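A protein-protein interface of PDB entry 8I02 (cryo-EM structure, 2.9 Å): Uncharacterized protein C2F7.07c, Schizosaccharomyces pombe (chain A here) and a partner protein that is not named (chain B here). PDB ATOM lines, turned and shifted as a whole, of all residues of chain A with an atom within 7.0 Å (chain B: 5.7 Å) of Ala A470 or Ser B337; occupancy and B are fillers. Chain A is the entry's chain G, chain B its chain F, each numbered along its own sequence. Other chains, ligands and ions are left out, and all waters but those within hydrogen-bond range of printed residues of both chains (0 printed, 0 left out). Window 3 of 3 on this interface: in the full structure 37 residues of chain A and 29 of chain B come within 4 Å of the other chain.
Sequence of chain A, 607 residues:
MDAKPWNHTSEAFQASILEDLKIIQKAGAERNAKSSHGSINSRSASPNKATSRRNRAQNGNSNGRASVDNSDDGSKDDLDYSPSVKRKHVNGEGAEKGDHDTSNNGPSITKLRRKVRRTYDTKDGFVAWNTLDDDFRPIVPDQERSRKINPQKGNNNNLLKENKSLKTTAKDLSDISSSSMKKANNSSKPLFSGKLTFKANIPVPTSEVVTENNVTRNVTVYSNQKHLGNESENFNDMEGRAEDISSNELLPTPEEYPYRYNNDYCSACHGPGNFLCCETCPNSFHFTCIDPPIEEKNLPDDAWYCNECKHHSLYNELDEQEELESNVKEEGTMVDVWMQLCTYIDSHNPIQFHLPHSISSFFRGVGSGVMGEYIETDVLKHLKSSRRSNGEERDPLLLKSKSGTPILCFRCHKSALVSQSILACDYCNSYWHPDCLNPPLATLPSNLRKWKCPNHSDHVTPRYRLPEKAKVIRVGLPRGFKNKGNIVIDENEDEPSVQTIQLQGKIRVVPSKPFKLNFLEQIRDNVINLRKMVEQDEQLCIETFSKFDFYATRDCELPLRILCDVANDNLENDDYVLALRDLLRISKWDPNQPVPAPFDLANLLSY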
ATOM      1  N   ARG A 364      34.944  31.659   2.829  1.00  0.00           N
ATOM      2  CA  ARG A 364      34.558  33.004   2.438  1.00  0.00           C
ATOM      3  C   ARG A 364      35.292  34.016   3.305  1.00  0.00           C
ATOM      4  O   ARG A 364      35.267  33.920   4.533  1.00  0.00           O
ATOM      5  CB  ARG A 364      33.047  33.185   2.578  1.00  0.00           C
ATOM      6  CG  ARG A 364      32.424  34.138   1.584  1.00  0.00           C
ATOM      7  CD  ARG A 364      32.849  33.792   0.173  1.00  0.00           C
ATOM      8  NE  ARG A 364      32.172  34.599  -0.837  1.00  0.00           N
ATOM      9  CZ  ARG A 364      31.184  34.162  -1.611  1.00  0.00           C
ATOM     10  NH1 ARG A 364      30.744  32.917  -1.502  1.00  0.00           N
ATOM     11  NH2 ARG A 364      30.634  34.974  -2.500  1.00  0.00           N
ATOM     12  N   ARG A 465      31.932  29.487   8.833  1.00  0.00           N
ATOM     13  CA  ARG A 465      32.578  29.920   7.603  1.00  0.00           C
ATOM     14  C   ARG A 465      32.002  29.158   6.420  1.00  0.00           C
ATOM     15  O   ARG A 465      31.751  27.954   6.509  1.00  0.00           O
ATOM     16  CB  ARG A 465      34.094  29.718   7.671  1.00  0.00           C
ATOM     17  CG  ARG A 465      34.539  28.677   8.675  1.00  0.00           C
ATOM     18  CD  ARG A 465      36.045  28.577   8.751  1.00  0.00           C
ATOM     19  NE  ARG A 465      36.674  29.796   9.246  1.00  0.00           N
ATOM     20  CZ  ARG A 465      37.960  29.888   9.562  1.00  0.00           C
ATOM     21  NH1 ARG A 465      38.744  28.838   9.437  1.00  0.00           N
ATOM     22  NH2 ARG A 465      38.460  31.026  10.001  1.00  0.00           N
ATOM     23  N   LEU A 466      31.808  29.861   5.311  1.00  0.00           N
ATOM     24  CA  LEU A 466      31.078  29.309   4.183  1.00  0.00           C
ATOM     25  C   LEU A 466      32.012  28.891   3.063  1.00  0.00           C
ATOM     26  O   LEU A 466      32.951  29.613   2.743  1.00  0.00           O
ATOM     27  CB  LEU A 466      30.086  30.330   3.634  1.00  0.00           C
ATOM     28  CG  LEU A 466      28.881  30.713   4.474  1.00  0.00           C
ATOM     29  CD1 LEU A 466      28.016  31.634   3.663  1.00  0.00           C
ATOM     30  CD2 LEU A 466      28.121  29.488   4.872  1.00  0.00           C
ATOM     31  N   PRO A 467      31.728  27.786   2.410  1.00  0.00           N
ATOM     32  CA  PRO A 467      32.654  27.241   1.414  1.00  0.00           C
ATOM     33  C   PRO A 467      32.899  28.100   0.181  1.00  0.00           C
ATOM     34  O   PRO A 467      33.488  27.606  -0.785  1.00  0.00           O
ATOM     35  CB  PRO A 467      31.992  25.916   1.037  1.00  0.00           C
ATOM     36  CG  PRO A 467      31.237  25.550   2.230  1.00  0.00           C
ATOM     37  CD  PRO A 467      30.688  26.815   2.760  1.00  0.00           C
ATOM     38  N   GLU A 468      32.405  29.337   0.153  1.00  0.00           N
ATOM     39  CA  GLU A 468      32.811  30.318  -0.850  1.00  0.00           C
ATOM     40  C   GLU A 468      32.316  29.963  -2.242  1.00  0.00           C
ATOM     41  O   GLU A 468      32.475  30.743  -3.185  1.00  0.00           O
ATOM     42  CB  GLU A 468      34.335  30.471  -0.871  1.00  0.00           C
ATOM     43  CG  GLU A 468      34.871  31.682  -1.622  1.00  0.00           C
ATOM     44  CD  GLU A 468      35.428  31.350  -2.988  1.00  0.00           C
ATOM     45  OE1 GLU A 468      35.882  30.206  -3.193  1.00  0.00           O
ATOM     46  OE2 GLU A 468      35.410  32.242  -3.857  1.00  0.00           O
ATOM     47  N   LYS A 469      31.712  28.799  -2.392  1.00  0.00           N
ATOM     48  CA  LYS A 469      31.032  28.459  -3.631  1.00  0.00           C
ATOM     49  C   LYS A 469      29.717  27.765  -3.335  1.00  0.00           C
ATOM     50  O   LYS A 469      29.090  27.234  -4.256  1.00  0.00           O
ATOM     51  CB  LYS A 469      31.907  27.589  -4.534  1.00  0.00           C
ATOM     52  CG  LYS A 469      32.919  28.375  -5.330  1.00  0.00           C
ATOM     53  CD  LYS A 469      33.998  27.477  -5.885  1.00  0.00           C
ATOM     54  CE  LYS A 469      33.421  26.378  -6.750  1.00  0.00           C
ATOM     55  NZ  LYS A 469      34.496  25.549  -7.361  1.00  0.00           N
ATOM     56  N   ALA A 470      29.302  27.737  -2.079  1.00  0.00           N
ATOM     57  CA  ALA A 470      27.964  27.313  -1.738  1.00  0.00           C
ATOM     58  C   ALA A 470      26.944  28.225  -2.410  1.00  0.00           C
ATOM     59  O   ALA A 470      27.244  29.352  -2.810  1.00  0.00           O
ATOM     60  CB  ALA A 470      27.776  27.332  -0.222  1.00  0.00           C
ATOM     61  N   LYS A 471      25.729  27.719  -2.545  1.00  0.00           N
ATOM     62  CA  LYS A 471      24.606  28.497  -3.031  1.00  0.00           C
ATOM     63  C   LYS A 471      23.604  28.691  -1.903  1.00  0.00           C
ATOM     64  O   LYS A 471      23.773  28.185  -0.791  1.00  0.00           O
ATOM     65  CB  LYS A 471      23.956  27.820  -4.234  1.00  0.00           C
ATOM     66  CG  LYS A 471      24.867  27.673  -5.422  1.00  0.00           C
ATOM     67  CD  LYS A 471      24.942  26.231  -5.858  1.00  0.00           C
ATOM     68  CE  LYS A 471      25.542  25.364  -4.768  1.00  0.00           C
ATOM     69  NZ  LYS A 471      25.847  23.998  -5.256  1.00  0.00           N
ATOM     70  N   VAL A 472      22.554  29.442  -2.201  1.00  0.00           N
ATOM     71  CA  VAL A 472      21.475  29.679  -1.254  1.00  0.00           C
ATOM     72  C   VAL A 472      20.368  28.676  -1.543  1.00  0.00           C
ATOM     73  O   VAL A 472      19.791  28.672  -2.633  1.00  0.00           O
ATOM     74  CB  VAL A 472      20.959  31.120  -1.352  1.00  0.00           C
ATOM     75  CG1 VAL A 472      20.814  31.713   0.024  1.00  0.00           C
ATOM     76  CG2 VAL A 472      21.904  31.951  -2.182  1.00  0.00           C
ATOM     77  N   ASN A 486      22.333  30.747   9.757  1.00  0.00           N
ATOM     78  CA  ASN A 486      22.906  30.902   8.426  1.00  0.00           C
ATOM     79  C   ASN A 486      21.844  31.190   7.369  1.00  0.00           C
ATOM     80  O   ASN A 486      21.907  30.673   6.257  1.00  0.00           O
ATOM     81  CB  ASN A 486      23.726  29.673   8.037  1.00  0.00           C
ATOM     82  CG  ASN A 486      23.375  28.436   8.848  1.00  0.00           C
ATOM     83  OD1 ASN A 486      22.801  27.492   8.330  1.00  0.00           O
ATOM     84  ND2 ASN A 486      23.755  28.424  10.112  1.00  0.00           N
ATOM     85  N   LEU B 334      30.613  19.104   6.929  1.00  0.00           N
ATOM     86  CA  LEU B 334      30.684  20.462   7.443  1.00  0.00           C
ATOM     87  C   LEU B 334      29.446  20.778   8.272  1.00  0.00           C
ATOM     88  O   LEU B 334      28.338  20.367   7.914  1.00  0.00           O
ATOM     89  CB  LEU B 334      30.805  21.464   6.298  1.00  0.00           C
ATOM     90  CG  LEU B 334      32.137  21.613   5.578  1.00  0.00           C
ATOM     91  CD1 LEU B 334      31.976  22.568   4.441  1.00  0.00           C
ATOM     92  CD2 LEU B 334      33.184  22.121   6.522  1.00  0.00           C
ATOM     93  N   PRO B 335      29.593  21.501   9.384  1.00  0.00           N
ATOM     94  CA  PRO B 335      28.412  21.872  10.171  1.00  0.00           C
ATOM     95  C   PRO B 335      27.601  22.994   9.555  1.00  0.00           C
ATOM     96  O   PRO B 335      26.421  23.135   9.899  1.00  0.00           O
ATOM     97  CB  PRO B 335      29.008  22.290  11.519  1.00  0.00           C
ATOM     98  CG  PRO B 335      30.369  22.755  11.186  1.00  0.00           C
ATOM     99  CD  PRO B 335      30.844  21.930  10.025  1.00  0.00           C
ATOM    100  N   VAL B 336      28.189  23.791   8.663  1.00  0.00           N
ATOM    101  CA  VAL B 336      27.499  24.859   7.949  1.00  0.00           C
ATOM    102  C   VAL B 336      27.986  24.816   6.510  1.00  0.00           C
ATOM    103  O   VAL B 336      29.122  25.204   6.226  1.00  0.00           O
ATOM    104  CB  VAL B 336      27.755  26.241   8.561  1.00  0.00           C
ATOM    105  CG1 VAL B 336      27.328  27.314   7.611  1.00  0.00           C
ATOM    106  CG2 VAL B 336      27.018  26.379   9.870  1.00  0.00           C
ATOM    107  N   SER B 337      27.144  24.337   5.605  1.00  0.00           N
ATOM    108  CA  SER B 337      27.545  24.123   4.227  1.00  0.00           C
ATOM    109  C   SER B 337      26.962  25.133   3.257  1.00  0.00           C
ATOM    110  O   SER B 337      27.416  25.185   2.110  1.00  0.00           O
ATOM    111  CB  SER B 337      27.144  22.717   3.772  1.00  0.00           C
ATOM    112  OG  SER B 337      27.213  21.798   4.850  1.00  0.00           O
ATOM    113  N   CYS B 338      25.970  25.918   3.673  1.00  0.00           N
ATOM    114  CA  CYS B 338      25.291  26.851   2.778  1.00  0.00           C
ATOM    115  C   CYS B 338      24.468  27.829   3.607  1.00  0.00           C
ATOM    116  O   CYS B 338      24.392  27.734   4.837  1.00  0.00           O
ATOM    117  CB  CYS B 338      24.393  26.117   1.783  1.00  0.00           C
ATOM    118  SG  CYS B 338      23.271  24.938   2.547  1.00  0.00           S
ATOM    119  N   LEU B 339      23.857  28.779   2.908  1.00  0.00           N
ATOM    120  CA  LEU B 339      22.866  29.693   3.449  1.00  0.00           C
ATOM    121  C   LEU B 339      21.473  29.239   3.043  1.00  0.00           C
ATOM    122  O   LEU B 339      21.263  28.703   1.956  1.00  0.00           O
ATOM    123  CB  LEU B 339      23.093  31.119   2.947  1.00  0.00           C
ATOM    124  CG  LEU B 339      24.339  31.889   3.356  1.00  0.00           C
ATOM    125  CD1 LEU B 339      24.619  32.925   2.319  1.00  0.00           C
ATOM    126  CD2 LEU B 339      24.138  32.551   4.685  1.00  0.00           C
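The backbone NH of Arg A364 lies within hydrogen-bond range of the backbone carbonyl oxygen of Leu A466.
Among the printed residues, merely in contact across the chains: Arg A465 with Val B336, Leu A466 with Val B336, Leu A466 with Leu B339, Pro A467 with Leu B334, Pro A467 with Ser B337, Ala A470 with Ser B337, Ala A470 with Cys B338, Lys A471 with Cys B338, Lys A471 with Leu B339, Val A472 with Leu B339, Asn A486 with Val B336, Asn A486 with Cys B338 and Asn A486 with Leu B339.
Printed residues of chain A within 4 Å of Ser B337: Pro A467 (3.7 Å) and Ala A470 (3.2 Å). Printed residues of chain A within 4 Å of Leu B334: Pro A467. Of the printed residues of chain A, Val B336 touches Arg A465 (3.8 Å), Leu A466 (3.6 Å) and Asn A486 (3.9 Å). Of the printed residues of chain B, Leu A466 touches Val B336 (3.6 Å) and Leu B339 (3.7 Å).
Among the printed residues, no Asp or Glu carboxylate lies within 4 Å of a Lys or Arg side-chain nitrogen of the other chain.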
